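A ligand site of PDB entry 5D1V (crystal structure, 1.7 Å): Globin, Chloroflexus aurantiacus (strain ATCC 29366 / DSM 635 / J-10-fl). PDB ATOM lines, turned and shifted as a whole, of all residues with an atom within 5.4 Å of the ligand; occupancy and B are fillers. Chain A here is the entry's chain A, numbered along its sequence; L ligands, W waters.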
ATOM      1  N   TYR A  24       8.603 -25.304  31.059  1.00  0.00           N
ATOM      2  CA  TYR A  24       7.381 -25.471  31.833  1.00  0.00           C
ATOM      3  C   TYR A  24       7.438 -24.750  33.180  1.00  0.00           C
ATOM      4  O   TYR A  24       6.426 -24.243  33.664  1.00  0.00           O
ATOM      5  CB  TYR A  24       7.071 -26.949  32.013  1.00  0.00           C
ATOM      6  CG  TYR A  24       5.990 -27.393  31.049  1.00  0.00           C
ATOM      7  CD1 TYR A  24       6.278 -27.673  29.732  1.00  0.00           C
ATOM      8  CD2 TYR A  24       4.682 -27.473  31.458  1.00  0.00           C
ATOM      9  CE1 TYR A  24       5.288 -28.037  28.836  1.00  0.00           C
ATOM     10  CE2 TYR A  24       3.686 -27.829  30.592  1.00  0.00           C
ATOM     11  CZ  TYR A  24       3.983 -28.109  29.275  1.00  0.00           C
ATOM     12  OH  TYR A  24       2.987 -28.488  28.412  1.00  0.00           O
ATOM     13  N   LEU A  33       0.137 -17.085  30.525  1.00  0.00           N
ATOM     14  CA  LEU A  33      -0.002 -18.384  29.877  1.00  0.00           C
ATOM     15  C   LEU A  33      -0.682 -19.434  30.732  1.00  0.00           C
ATOM     16  O   LEU A  33      -1.402 -20.265  30.190  1.00  0.00           O
ATOM     17  CB  LEU A  33       1.352 -18.946  29.500  1.00  0.00           C
ATOM     18  CG  LEU A  33       2.042 -18.166  28.386  1.00  0.00           C
ATOM     19  CD1 LEU A  33       3.465 -18.713  28.180  1.00  0.00           C
ATOM     20  CD2 LEU A  33       1.255 -18.200  27.086  1.00  0.00           C
ATOM     21  N   LEU A  36      -4.202 -21.076  30.432  1.00  0.00           N
ATOM     22  CA  LEU A  36      -4.566 -21.825  29.240  1.00  0.00           C
ATOM     23  C   LEU A  36      -4.324 -23.306  29.395  1.00  0.00           C
ATOM     24  O   LEU A  36      -4.923 -24.120  28.670  1.00  0.00           O
ATOM     25  CB  LEU A  36      -3.767 -21.309  28.041  1.00  0.00           C
ATOM     26  CG  LEU A  36      -4.149 -19.903  27.547  1.00  0.00           C
ATOM     27  CD1 LEU A  36      -3.184 -19.458  26.417  1.00  0.00           C
ATOM     28  CD2 LEU A  36      -5.557 -19.862  27.082  1.00  0.00           C
ATOM     29  N   PHE A  37      -3.444 -23.654  30.329  1.00  0.00           N
ATOM     30  CA  PHE A  37      -3.019 -25.015  30.538  1.00  0.00           C
ATOM     31  C   PHE A  37      -3.896 -25.720  31.570  1.00  0.00           C
ATOM     32  O   PHE A  37      -4.519 -25.067  32.422  1.00  0.00           O
ATOM     33  CB  PHE A  37      -1.551 -25.044  30.999  1.00  0.00           C
ATOM     34  CG  PHE A  37      -0.556 -24.682  29.906  1.00  0.00           C
ATOM     35  CD1 PHE A  37      -0.345 -23.365  29.530  1.00  0.00           C
ATOM     36  CD2 PHE A  37       0.145 -25.676  29.260  1.00  0.00           C
ATOM     37  CE1 PHE A  37       0.547 -23.053  28.531  1.00  0.00           C
ATOM     38  CE2 PHE A  37       1.067 -25.349  28.246  1.00  0.00           C
ATOM     39  CZ  PHE A  37       1.258 -24.064  27.895  1.00  0.00           C
ATOM     40  N   PRO A  38      -3.941 -27.058  31.531  1.00  0.00           N
ATOM     41  CA  PRO A  38      -4.838 -27.755  32.465  1.00  0.00           C
ATOM     42  C   PRO A  38      -4.355 -27.673  33.908  1.00  0.00           C
ATOM     43  O   PRO A  38      -3.250 -27.217  34.159  1.00  0.00           O
ATOM     44  CB  PRO A  38      -4.814 -29.204  31.986  1.00  0.00           C
ATOM     45  CG  PRO A  38      -4.123 -29.194  30.645  1.00  0.00           C
ATOM     46  CD  PRO A  38      -3.256 -27.977  30.612  1.00  0.00           C
ATOM     47  N   ASP A  40      -3.445 -30.158  35.728  1.00  0.00           N
ATOM     48  CA  ASP A  40      -2.310 -31.075  35.808  1.00  0.00           C
ATOM     49  C   ASP A  40      -1.492 -30.886  34.540  1.00  0.00           C
ATOM     50  O   ASP A  40      -1.968 -31.181  33.433  1.00  0.00           O
ATOM     51  CB  ASP A  40      -2.766 -32.544  35.932  1.00  0.00           C
ATOM     52  CG  ASP A  40      -1.595 -33.540  35.998  1.00  0.00           C
ATOM     53  OD1 ASP A  40      -0.412 -33.112  35.958  1.00  0.00           O
ATOM     54  OD2 ASP A  40      -1.879 -34.760  36.119  1.00  0.00           O
ATOM     55  N   LEU A  41      -0.267 -30.401  34.684  1.00  0.00           N
ATOM     56  CA  LEU A  41       0.566 -30.104  33.511  1.00  0.00           C
ATOM     57  C   LEU A  41       1.308 -31.319  32.964  1.00  0.00           C
ATOM     58  O   LEU A  41       1.837 -31.251  31.871  1.00  0.00           O
ATOM     59  CB  LEU A  41       1.579 -29.015  33.850  1.00  0.00           C
ATOM     60  CG  LEU A  41       1.016 -27.666  34.323  1.00  0.00           C
ATOM     61  CD1 LEU A  41       2.150 -26.787  34.850  1.00  0.00           C
ATOM     62  CD2 LEU A  41       0.286 -26.943  33.226  1.00  0.00           C
ATOM     63  N   PRO A  43       0.824 -34.587  31.813  1.00  0.00           N
ATOM     64  CA  PRO A  43       0.654 -35.279  30.534  1.00  0.00           C
ATOM     65  C   PRO A  43       1.044 -34.436  29.326  1.00  0.00           C
ATOM     66  O   PRO A  43       1.710 -34.929  28.427  1.00  0.00           O
ATOM     67  CB  PRO A  43      -0.846 -35.601  30.491  1.00  0.00           C
ATOM     68  CG  PRO A  43      -1.284 -35.583  31.923  1.00  0.00           C
ATOM     69  CD  PRO A  43      -0.418 -34.579  32.621  1.00  0.00           C
ATOM     70  N   GLY A  44       0.638 -33.172  29.320  1.00  0.00           N
ATOM     71  CA  GLY A  44       0.956 -32.253  28.253  1.00  0.00           C
ATOM     72  C   GLY A  44       2.438 -31.955  28.146  1.00  0.00           C
ATOM     73  O   GLY A  44       2.980 -31.829  27.051  1.00  0.00           O
ATOM     74  N   LYS A  45       3.111 -31.865  29.296  1.00  0.00           N
ATOM     75  CA  LYS A  45       4.553 -31.676  29.336  1.00  0.00           C
ATOM     76  C   LYS A  45       5.270 -32.808  28.621  1.00  0.00           C
ATOM     77  O   LYS A  45       6.138 -32.546  27.787  1.00  0.00           O
ATOM     78  CB  LYS A  45       5.038 -31.544  30.783  1.00  0.00           C
ATOM     79  CG  LYS A  45       6.507 -31.281  30.940  1.00  0.00           C
ATOM     80  CD  LYS A  45       6.854 -31.233  32.447  1.00  0.00           C
ATOM     81  CE  LYS A  45       8.360 -31.078  32.619  1.00  0.00           C
ATOM     82  NZ  LYS A  45       8.864 -31.657  33.895  1.00  0.00           N
ATOM     83  N   HIS A  47       3.982 -34.818  26.401  1.00  0.00           N
ATOM     84  CA  HIS A  47       3.610 -34.770  24.991  1.00  0.00           C
ATOM     85  C   HIS A  47       4.454 -33.748  24.275  1.00  0.00           C
ATOM     86  O   HIS A  47       4.927 -33.999  23.165  1.00  0.00           O
ATOM     87  CB  HIS A  47       2.114 -34.459  24.808  1.00  0.00           C
ATOM     88  CG  HIS A  47       1.218 -35.568  25.276  1.00  0.00           C
ATOM     89  ND1 HIS A  47      -0.075 -35.354  25.700  1.00  0.00           N
ATOM     90  CD2 HIS A  47       1.453 -36.895  25.394  1.00  0.00           C
ATOM     91  CE1 HIS A  47      -0.602 -36.509  26.063  1.00  0.00           C
ATOM     92  NE2 HIS A  47       0.303 -37.462  25.887  1.00  0.00           N
ATOM     93  N   GLN A  48       4.676 -32.597  24.909  1.00  0.00           N
ATOM     94  CA  GLN A  48       5.474 -31.588  24.231  1.00  0.00           C
ATOM     95  C   GLN A  48       6.934 -32.073  24.065  1.00  0.00           C
ATOM     96  O   GLN A  48       7.531 -31.884  22.993  1.00  0.00           O
ATOM     97  CB  GLN A  48       5.464 -30.273  24.984  1.00  0.00           C
ATOM     98  CG  GLN A  48       6.095 -29.182  24.123  1.00  0.00           C
ATOM     99  CD  GLN A  48       6.414 -27.958  24.888  1.00  0.00           C
ATOM    100  OE1 GLN A  48       7.039 -28.033  25.947  1.00  0.00           O
ATOM    101  NE2 GLN A  48       5.979 -26.807  24.385  1.00  0.00           N
ATOM    102  N   PHE A  51       7.120 -34.585  21.257  1.00  0.00           N
ATOM    103  CA  PHE A  51       6.982 -33.915  19.981  1.00  0.00           C
ATOM    104  C   PHE A  51       8.312 -33.294  19.548  1.00  0.00           C
ATOM    105  O   PHE A  51       8.745 -33.487  18.419  1.00  0.00           O
ATOM    106  CB  PHE A  51       5.946 -32.807  19.993  1.00  0.00           C
ATOM    107  CG  PHE A  51       6.011 -31.965  18.759  1.00  0.00           C
ATOM    108  CD1 PHE A  51       5.623 -32.486  17.533  1.00  0.00           C
ATOM    109  CD2 PHE A  51       6.595 -30.704  18.785  1.00  0.00           C
ATOM    110  CE1 PHE A  51       5.742 -31.733  16.360  1.00  0.00           C
ATOM    111  CE2 PHE A  51       6.737 -29.945  17.641  1.00  0.00           C
ATOM    112  CZ  PHE A  51       6.308 -30.462  16.406  1.00  0.00           C
ATOM    113  N   LEU A  52       8.948 -32.535  20.446  1.00  0.00           N
ATOM    114  CA  LEU A  52      10.187 -31.890  20.093  1.00  0.00           C
ATOM    115  C   LEU A  52      11.235 -32.928  19.702  1.00  0.00           C
ATOM    116  O   LEU A  52      11.960 -32.780  18.710  1.00  0.00           O
ATOM    117  CB  LEU A  52      10.693 -31.016  21.234  1.00  0.00           C
ATOM    118  CG  LEU A  52       9.774 -29.832  21.551  1.00  0.00           C
ATOM    119  CD1 LEU A  52      10.218 -29.143  22.853  1.00  0.00           C
ATOM    120  CD2 LEU A  52       9.724 -28.833  20.400  1.00  0.00           C
ATOM    121  N   TYR A  62       6.225 -39.840  19.932  1.00  0.00           N
ATOM    122  CA  TYR A  62       5.105 -38.928  19.901  1.00  0.00           C
ATOM    123  C   TYR A  62       3.986 -39.472  19.004  1.00  0.00           C
ATOM    124  O   TYR A  62       2.819 -39.548  19.415  1.00  0.00           O
ATOM    125  CB  TYR A  62       5.527 -37.532  19.399  1.00  0.00           C
ATOM    126  CG  TYR A  62       4.334 -36.611  19.348  1.00  0.00           C
ATOM    127  CD1 TYR A  62       3.904 -35.923  20.472  1.00  0.00           C
ATOM    128  CD2 TYR A  62       3.620 -36.459  18.170  1.00  0.00           C
ATOM    129  CE1 TYR A  62       2.797 -35.116  20.423  1.00  0.00           C
ATOM    130  CE2 TYR A  62       2.521 -35.650  18.105  1.00  0.00           C
ATOM    131  CZ  TYR A  62       2.099 -34.990  19.223  1.00  0.00           C
ATOM    132  OH  TYR A  62       0.977 -34.196  19.136  1.00  0.00           O
ATOM    133  N   ARG A  66       0.257 -40.104  19.976  1.00  0.00           N
ATOM    134  CA  ARG A  66      -0.634 -39.005  19.652  1.00  0.00           C
ATOM    135  C   ARG A  66      -1.019 -38.872  18.190  1.00  0.00           C
ATOM    136  O   ARG A  66      -1.854 -38.042  17.849  1.00  0.00           O
ATOM    137  CB  ARG A  66       0.026 -37.688  20.085  1.00  0.00           C
ATOM    138  CG  ARG A  66       0.370 -37.625  21.559  1.00  0.00           C
ATOM    139  CD  ARG A  66      -0.831 -37.609  22.453  1.00  0.00           C
ATOM    140  NE  ARG A  66      -1.481 -36.299  22.510  1.00  0.00           N
ATOM    141  CZ  ARG A  66      -2.667 -36.083  23.084  1.00  0.00           C
ATOM    142  NH1 ARG A  66      -3.357 -37.081  23.645  1.00  0.00           N
ATOM    143  NH2 ARG A  66      -3.165 -34.851  23.086  1.00  0.00           N
ATOM    144  N   LEU A  71      -0.547 -29.486  14.999  1.00  0.00           N
ATOM    145  CA  LEU A  71      -0.444 -28.556  16.112  1.00  0.00           C
ATOM    146  C   LEU A  71      -1.411 -27.388  15.993  1.00  0.00           C
ATOM    147  O   LEU A  71      -2.074 -27.022  16.972  1.00  0.00           O
ATOM    148  CB  LEU A  71       0.976 -28.036  16.267  1.00  0.00           C
ATOM    149  CG  LEU A  71       2.060 -29.040  16.660  1.00  0.00           C
ATOM    150  CD1 LEU A  71       3.387 -28.336  16.902  1.00  0.00           C
ATOM    151  CD2 LEU A  71       1.649 -29.905  17.872  1.00  0.00           C
ATOM    152  N   ARG A  74      -4.626 -28.558  17.199  1.00  0.00           N
ATOM    153  CA  ARG A  74      -4.666 -28.856  18.622  1.00  0.00           C
ATOM    154  C   ARG A  74      -4.670 -27.605  19.462  1.00  0.00           C
ATOM    155  O   ARG A  74      -5.090 -27.652  20.622  1.00  0.00           O
ATOM    156  CB  ARG A  74      -3.501 -29.738  19.056  1.00  0.00           C
ATOM    157  CG  ARG A  74      -3.500 -31.149  18.544  1.00  0.00           C
ATOM    158  CD  ARG A  74      -2.311 -31.893  19.139  1.00  0.00           C
ATOM    159  NE  ARG A  74      -1.992 -33.112  18.414  1.00  0.00           N
ATOM    160  CZ  ARG A  74      -2.454 -34.313  18.739  1.00  0.00           C
ATOM    161  NH1 ARG A  74      -3.267 -34.477  19.764  1.00  0.00           N
ATOM    162  NH2 ARG A  74      -2.095 -35.348  18.022  1.00  0.00           N
ATOM    163  N   HIS A  75      -4.216 -26.481  18.902  1.00  0.00           N
ATOM    164  CA  HIS A  75      -4.159 -25.245  19.660  1.00  0.00           C
ATOM    165  C   HIS A  75      -5.411 -24.387  19.454  1.00  0.00           C
ATOM    166  O   HIS A  75      -5.558 -23.355  20.083  1.00  0.00           O
ATOM    167  CB  HIS A  75      -2.910 -24.428  19.316  1.00  0.00           C
ATOM    168  CG  HIS A  75      -1.657 -24.994  19.873  1.00  0.00           C
ATOM    169  ND1 HIS A  75      -1.078 -26.161  19.389  1.00  0.00           N
ATOM    170  CD2 HIS A  75      -0.873 -24.578  20.896  1.00  0.00           C
ATOM    171  CE1 HIS A  75       0.043 -26.399  20.077  1.00  0.00           C
ATOM    172  NE2 HIS A  75       0.165 -25.472  20.998  1.00  0.00           N
ATOM    173  N   PHE A  78      -7.393 -22.692  22.382  1.00  0.00           N
ATOM    174  CA  PHE A  78      -6.698 -21.664  23.161  1.00  0.00           C
ATOM    175  C   PHE A  78      -6.701 -20.339  22.393  1.00  0.00           C
ATOM    176  O   PHE A  78      -6.165 -20.283  21.282  1.00  0.00           O
ATOM    177  CB  PHE A  78      -5.256 -22.089  23.447  1.00  0.00           C
ATOM    178  CG  PHE A  78      -5.136 -23.509  23.854  1.00  0.00           C
ATOM    179  CD1 PHE A  78      -5.946 -24.025  24.864  1.00  0.00           C
ATOM    180  CD2 PHE A  78      -4.236 -24.369  23.227  1.00  0.00           C
ATOM    181  CE1 PHE A  78      -5.875 -25.361  25.237  1.00  0.00           C
ATOM    182  CE2 PHE A  78      -4.166 -25.688  23.589  1.00  0.00           C
ATOM    183  CZ  PHE A  78      -4.997 -26.200  24.588  1.00  0.00           C
ATOM    184  N   ILE A  80      -5.126 -17.472  21.050  1.00  0.00           N
ATOM    185  CA  ILE A  80      -3.705 -17.160  20.931  1.00  0.00           C
ATOM    186  C   ILE A  80      -3.550 -15.995  20.017  1.00  0.00           C
ATOM    187  O   ILE A  80      -3.825 -16.095  18.819  1.00  0.00           O
ATOM    188  CB  ILE A  80      -2.897 -18.345  20.428  1.00  0.00           C
ATOM    189  CG1 ILE A  80      -2.983 -19.496  21.420  1.00  0.00           C
ATOM    190  CG2 ILE A  80      -1.451 -17.952  20.231  1.00  0.00           C
ATOM    191  CD1 ILE A  80      -2.344 -20.770  20.876  1.00  0.00           C
ATOM    192  N   GLU A  84       0.226 -13.877  23.592  1.00  0.00           N
ATOM    193  CA  GLU A  84       0.454 -15.265  23.952  1.00  0.00           C
ATOM    194  C   GLU A  84       1.641 -15.823  23.154  1.00  0.00           C
ATOM    195  O   GLU A  84       2.476 -16.588  23.655  1.00  0.00           O
ATOM    196  CB  GLU A  84      -0.809 -16.102  23.702  1.00  0.00           C
ATOM    197  CG  GLU A  84      -1.952 -15.852  24.665  1.00  0.00           C
ATOM    198  CD  GLU A  84      -2.696 -14.561  24.414  1.00  0.00           C
ATOM    199  OE1 GLU A  84      -2.814 -14.141  23.246  1.00  0.00           O
ATOM    200  OE2 GLU A  84      -3.176 -13.923  25.387  1.00  0.00           O
ATOM    201  N   ARG A  85       1.722 -15.439  21.886  1.00  0.00           N
ATOM    202  CA  ARG A  85       2.852 -15.816  21.040  1.00  0.00           C
ATOM    203  C   ARG A  85       4.150 -15.359  21.680  1.00  0.00           C
ATOM    204  O   ARG A  85       5.125 -16.135  21.801  1.00  0.00           O
ATOM    205  CB  ARG A  85       2.698 -15.198  19.644  1.00  0.00           C
ATOM    206  CG  ARG A  85       3.826 -15.461  18.643  1.00  0.00           C
ATOM    207  CD  ARG A  85       3.839 -14.372  17.557  1.00  0.00           C
ATOM    208  NE  ARG A  85       3.923 -13.028  18.148  1.00  0.00           N
ATOM    209  CZ  ARG A  85       3.548 -11.897  17.554  1.00  0.00           C
ATOM    210  NH1 ARG A  85       3.051 -11.908  16.318  1.00  0.00           N
ATOM    211  NH2 ARG A  85       3.677 -10.736  18.171  1.00  0.00           N
ATOM    212  N   TRP A  88       5.053 -17.272  24.951  1.00  0.00           N
ATOM    213  CA  TRP A  88       5.555 -18.592  24.658  1.00  0.00           C
ATOM    214  C   TRP A  88       7.011 -18.556  24.138  1.00  0.00           C
ATOM    215  O   TRP A  88       7.906 -19.275  24.614  1.00  0.00           O
ATOM    216  CB  TRP A  88       4.630 -19.245  23.638  1.00  0.00           C
ATOM    217  CG  TRP A  88       4.841 -20.696  23.504  1.00  0.00           C
ATOM    218  CD1 TRP A  88       4.105 -21.682  24.087  1.00  0.00           C
ATOM    219  CD2 TRP A  88       5.845 -21.364  22.728  1.00  0.00           C
ATOM    220  NE1 TRP A  88       4.574 -22.905  23.725  1.00  0.00           N
ATOM    221  CE2 TRP A  88       5.650 -22.747  22.905  1.00  0.00           C
ATOM    222  CE3 TRP A  88       6.881 -20.923  21.890  1.00  0.00           C
ATOM    223  CZ2 TRP A  88       6.455 -23.702  22.280  1.00  0.00           C
ATOM    224  CZ3 TRP A  88       7.688 -21.881  21.278  1.00  0.00           C
ATOM    225  CH2 TRP A  88       7.468 -23.250  21.497  1.00  0.00           C
ATOM    226  N   TYR A 112      12.777 -22.501  13.774  1.00  0.00           N
ATOM    227  CA  TYR A 112      11.557 -23.274  13.716  1.00  0.00           C
ATOM    228  C   TYR A 112      10.500 -22.690  14.682  1.00  0.00           C
ATOM    229  O   TYR A 112       9.342 -22.476  14.313  1.00  0.00           O
ATOM    230  CB  TYR A 112      11.828 -24.736  14.033  1.00  0.00           C
ATOM    231  CG  TYR A 112      10.529 -25.461  14.337  1.00  0.00           C
ATOM    232  CD1 TYR A 112       9.641 -25.763  13.328  1.00  0.00           C
ATOM    233  CD2 TYR A 112      10.193 -25.770  15.640  1.00  0.00           C
ATOM    234  CE1 TYR A 112       8.435 -26.381  13.611  1.00  0.00           C
ATOM    235  CE2 TYR A 112       8.999 -26.392  15.936  1.00  0.00           C
ATOM    236  CZ  TYR A 112       8.119 -26.700  14.917  1.00  0.00           C
ATOM    237  OH  TYR A 112       6.918 -27.297  15.234  1.00  0.00           O
ATOM    238  N   PHE A 113      10.919 -22.397  15.918  1.00  0.00           N
ATOM    239  CA  PHE A 113       9.995 -21.906  16.937  1.00  0.00           C
ATOM    240  C   PHE A 113       9.381 -20.560  16.561  1.00  0.00           C
ATOM    241  O   PHE A 113       8.191 -20.309  16.815  1.00  0.00           O
ATOM    242  CB  PHE A 113      10.720 -21.797  18.282  1.00  0.00           C
ATOM    243  CG  PHE A 113      11.013 -23.117  18.935  1.00  0.00           C
ATOM    244  CD1 PHE A 113      10.083 -24.131  18.955  1.00  0.00           C
ATOM    245  CD2 PHE A 113      12.246 -23.335  19.537  1.00  0.00           C
ATOM    246  CE1 PHE A 113      10.367 -25.349  19.581  1.00  0.00           C
ATOM    247  CE2 PHE A 113      12.530 -24.546  20.158  1.00  0.00           C
ATOM    248  CZ  PHE A 113      11.592 -25.546  20.182  1.00  0.00           C
ATOM    249  N   ALA A 116       6.746 -21.320  13.935  1.00  0.00           N
ATOM    250  CA  ALA A 116       5.652 -22.113  14.481  1.00  0.00           C
ATOM    251  C   ALA A 116       4.766 -21.291  15.440  1.00  0.00           C
ATOM    252  O   ALA A 116       3.520 -21.404  15.420  1.00  0.00           O
ATOM    253  CB  ALA A 116       6.198 -23.309  15.188  1.00  0.00           C
ATOM    254  N   ALA A 117       5.407 -20.485  16.283  1.00  0.00           N
ATOM    255  CA  ALA A 117       4.663 -19.650  17.239  1.00  0.00           C
ATOM    256  C   ALA A 117       3.773 -18.642  16.507  1.00  0.00           C
ATOM    257  O   ALA A 117       2.649 -18.414  16.910  1.00  0.00           O
ATOM    258  CB  ALA A 117       5.592 -18.934  18.172  1.00  0.00           C
ATOM    259  N   MET A 120       0.741 -20.385  14.905  1.00  0.00           N
ATOM    260  CA  MET A 120      -0.207 -20.930  15.857  1.00  0.00           C
ATOM    261  C   MET A 120      -1.302 -19.922  16.203  1.00  0.00           C
ATOM    262  O   MET A 120      -2.331 -20.271  16.792  1.00  0.00           O
ATOM    263  CB  MET A 120       0.504 -21.369  17.123  1.00  0.00           C
ATOM    264  CG  MET A 120      -0.090 -22.544  17.794  1.00  0.00           C
ATOM    265  SD  MET A 120       0.178 -24.043  16.813  1.00  0.00           S
ATOM    266  CE  MET A 120       1.852 -24.453  17.284  1.00  0.00           C
HETATM  267  C1  LIG L   1       0.127 -28.220  23.747  1.00  0.00           C
HETATM  268  C2  LIG L   1       3.902 -27.401  20.803  1.00  0.00           C
HETATM  269  C3  LIG L   1       2.794 -22.653  20.758  1.00  0.00           C
HETATM  270  C4  LIG L   1      -0.136 -23.462  24.533  1.00  0.00           C
HETATM  271  C5  LIG L   1       1.196 -28.423  22.919  1.00  0.00           C
HETATM  272  C6  LIG L   1       1.714 -29.704  22.480  1.00  0.00           C
HETATM  273  C7  LIG L   1       2.744 -29.472  21.667  1.00  0.00           C
HETATM  274  C8  LIG L   1       2.928 -28.029  21.549  1.00  0.00           C
HETATM  275  C9  LIG L   1       3.684 -30.473  20.909  1.00  0.00           C
HETATM  276  C10 LIG L   1       1.116 -31.066  22.913  1.00  0.00           C
HETATM  277  C11 LIG L   1       0.279 -31.564  21.722  1.00  0.00           C
HETATM  278  C12 LIG L   1      -0.486 -32.811  22.153  1.00  0.00           C
HETATM  279  O1  LIG L   1      -1.406 -32.703  22.997  1.00  0.00           O
HETATM  280  O2  LIG L   1      -0.187 -33.912  21.654  1.00  0.00           O
HETATM  281  C13 LIG L   1       3.922 -26.046  20.513  1.00  0.00           C
HETATM  282  C14 LIG L   1       4.810 -25.374  19.596  1.00  0.00           C
HETATM  283  C15 LIG L   1       4.466 -24.063  19.587  1.00  0.00           C
HETATM  284  C16 LIG L   1       3.397 -23.868  20.516  1.00  0.00           C
HETATM  285  C17 LIG L   1       5.929 -26.079  18.793  1.00  0.00           C
HETATM  286  C18 LIG L   1       5.062 -22.861  18.827  1.00  0.00           C
HETATM  287  C19 LIG L   1       6.264 -22.987  18.265  1.00  0.00           C
HETATM  288  C20 LIG L   1       1.918 -22.437  21.790  1.00  0.00           C
HETATM  289  C21 LIG L   1       1.401 -21.141  22.231  1.00  0.00           C
HETATM  290  C22 LIG L   1       0.586 -21.411  23.277  1.00  0.00           C
HETATM  291  C23 LIG L   1       0.581 -22.827  23.544  1.00  0.00           C
HETATM  292  C24 LIG L   1       1.740 -19.784  21.539  1.00  0.00           C
HETATM  293  C25 LIG L   1      -0.180 -20.413  24.156  1.00  0.00           C
HETATM  294  C26 LIG L   1       0.387 -19.209  24.244  1.00  0.00           C
HETATM  295  C27 LIG L   1      -0.379 -24.807  24.621  1.00  0.00           C
HETATM  296  C28 LIG L   1      -1.330 -25.475  25.509  1.00  0.00           C
HETATM  297  C29 LIG L   1      -1.255 -26.807  25.270  1.00  0.00           C
HETATM  298  C30 LIG L   1      -0.258 -27.005  24.245  1.00  0.00           C
HETATM  299  C31 LIG L   1      -2.247 -24.762  26.505  1.00  0.00           C
HETATM  300  C32 LIG L   1      -2.058 -27.925  25.946  1.00  0.00           C
HETATM  301  C33 LIG L   1      -1.207 -28.487  27.067  1.00  0.00           C
HETATM  302  C34 LIG L   1      -1.888 -29.633  27.768  1.00  0.00           C
HETATM  303  O3  LIG L   1      -1.429 -29.970  28.885  1.00  0.00           O
HETATM  304  O4  LIG L   1      -2.877 -30.177  27.223  1.00  0.00           O
HETATM  305  N1  LIG L   1       1.951 -27.426  22.315  1.00  0.00           N
HETATM  306  N2  LIG L   1       3.066 -25.103  21.046  1.00  0.00           N
HETATM  307  N3  LIG L   1       1.367 -23.419  22.595  1.00  0.00           N
HETATM  308  N4  LIG L   1       0.241 -25.782  23.878  1.00  0.00           N
HETATM  309 FE1  LIG L   1       1.669 -25.406  22.491  1.00  0.00          FE
HETATM  310  O   HOH W   1      -3.309 -32.933  27.182  1.00  0.00           O
HETATM  311  O   HOH W   2      -5.548 -28.968  27.157  1.00  0.00           O
HETATM  312  O   HOH W   3      -1.525 -31.911  30.760  1.00  0.00           O
HETATM  313  O   HOH W   4      -0.939 -32.351  25.487  1.00  0.00           O
HETATM  314  O   HOH W   5       0.745 -29.236  29.969  1.00  0.00           O
HETATM  315  O   HOH W   6       3.103 -25.401  24.114  1.00  0.00           O
HETATM  316  O   HOH W   7       1.416 -29.980  25.878  1.00  0.00           O
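Water W6 bridges NE1 of Trp 88 (2.9 Å) and NE2 of Gln 48 (3.2 Å).
Water W5 lies within hydrogen-bond range of an oxygen (O3) of the ligand (2.5 Å), the side-chain hydroxyl (OH) of Tyr 24 (2.8 Å) and the backbone carbonyl oxygen (O) of Leu 41 (3.0 Å).
Water W4 lies within hydrogen-bond range of O1 of the ligand (2.6 Å) and ND1 of His 47 (3.1 Å).
Water W3 lies within hydrogen-bond range of an oxygen (O3) of the ligand (2.7 Å), the backbone carbonyl oxygen of Asp 40 (2.8 Å) and the backbone NH of Gly 44 (2.9 Å).
Water W7 bridges the backbone carbonyl oxygen (O) of Gly 44 (2.7 Å) and the side-chain hydroxyl (OH) of Tyr 24 (3.3 Å).
A ring nitrogen (NE2) of His 75 binds an iron atom (FE1) of the ligand (2.1 Å).
An oxygen (O1) of the ligand is in salt-bridge range of the guanidinium group (NH2) of Arg 66, 2.8 Å away.
An oxygen (O2) of the ligand lies within hydrogen-bond range of the side-chain hydroxyl (OH) of Tyr 62, at 2.8 Å.
An oxygen (O2) of the ligand is in salt-bridge range of the guanidinium group of Arg 74, at 3.7 Å.
ND1 of His 75 sits at hydrogen-bond distance from SD of Met 120 (3.6 Å).
ND1 of His 75 sits at hydrogen-bond distance from O of Leu 71.
The backbone carbonyl oxygen (O) of Arg 66 is in hydrogen-bond range of the guanidinium group (NH2) of Arg 74 (2.7 Å).
OH of Tyr 62 is in hydrogen-bond range of NE of Arg 74, at 3.2 Å.
A ring nitrogen (ND1) of His 47 sits close to the backbone carbonyl oxygen (O) of Pro 43, at 3.3 Å.
A nitrogen (N3) of the ligand lies close to the indole nitrogen (NE1) of Trp 88, at 3.4 Å.
Leu 33 touches the ligand.
Leu 36 touches the ligand.
Phe 37 touches the ligand.
CD of Pro 38 touches O3 of the ligand, 3.2 Å away.
Gly 44 touches the ligand (CA to O3, 3.4 Å).
CB of His 47 touches O2 of the ligand (3.9 Å).
Gln 48 touches the ligand.
Phe 51 touches the ligand (CB to C9, 3.4 Å).
Leu 71 touches the ligand.
CE2 of Phe 78 touches C28 of the ligand (3.4 Å).
CD1 of Ile 80 touches C22 of the ligand, at 3.8 Å.
Glu 84 touches the ligand.
Tyr 112 touches the ligand.
Phe 113 touches the ligand.
Ala 116 touches the ligand.
N of Ala 117 touches C19 of the ligand (3.3 Å).
Met 120 touches the ligand.
Of the 29 residues printed, 22 come within 4 Å of the ligand.
The nearest printed residue that does not touch the ligand is Arg 85 (4.2 Å).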
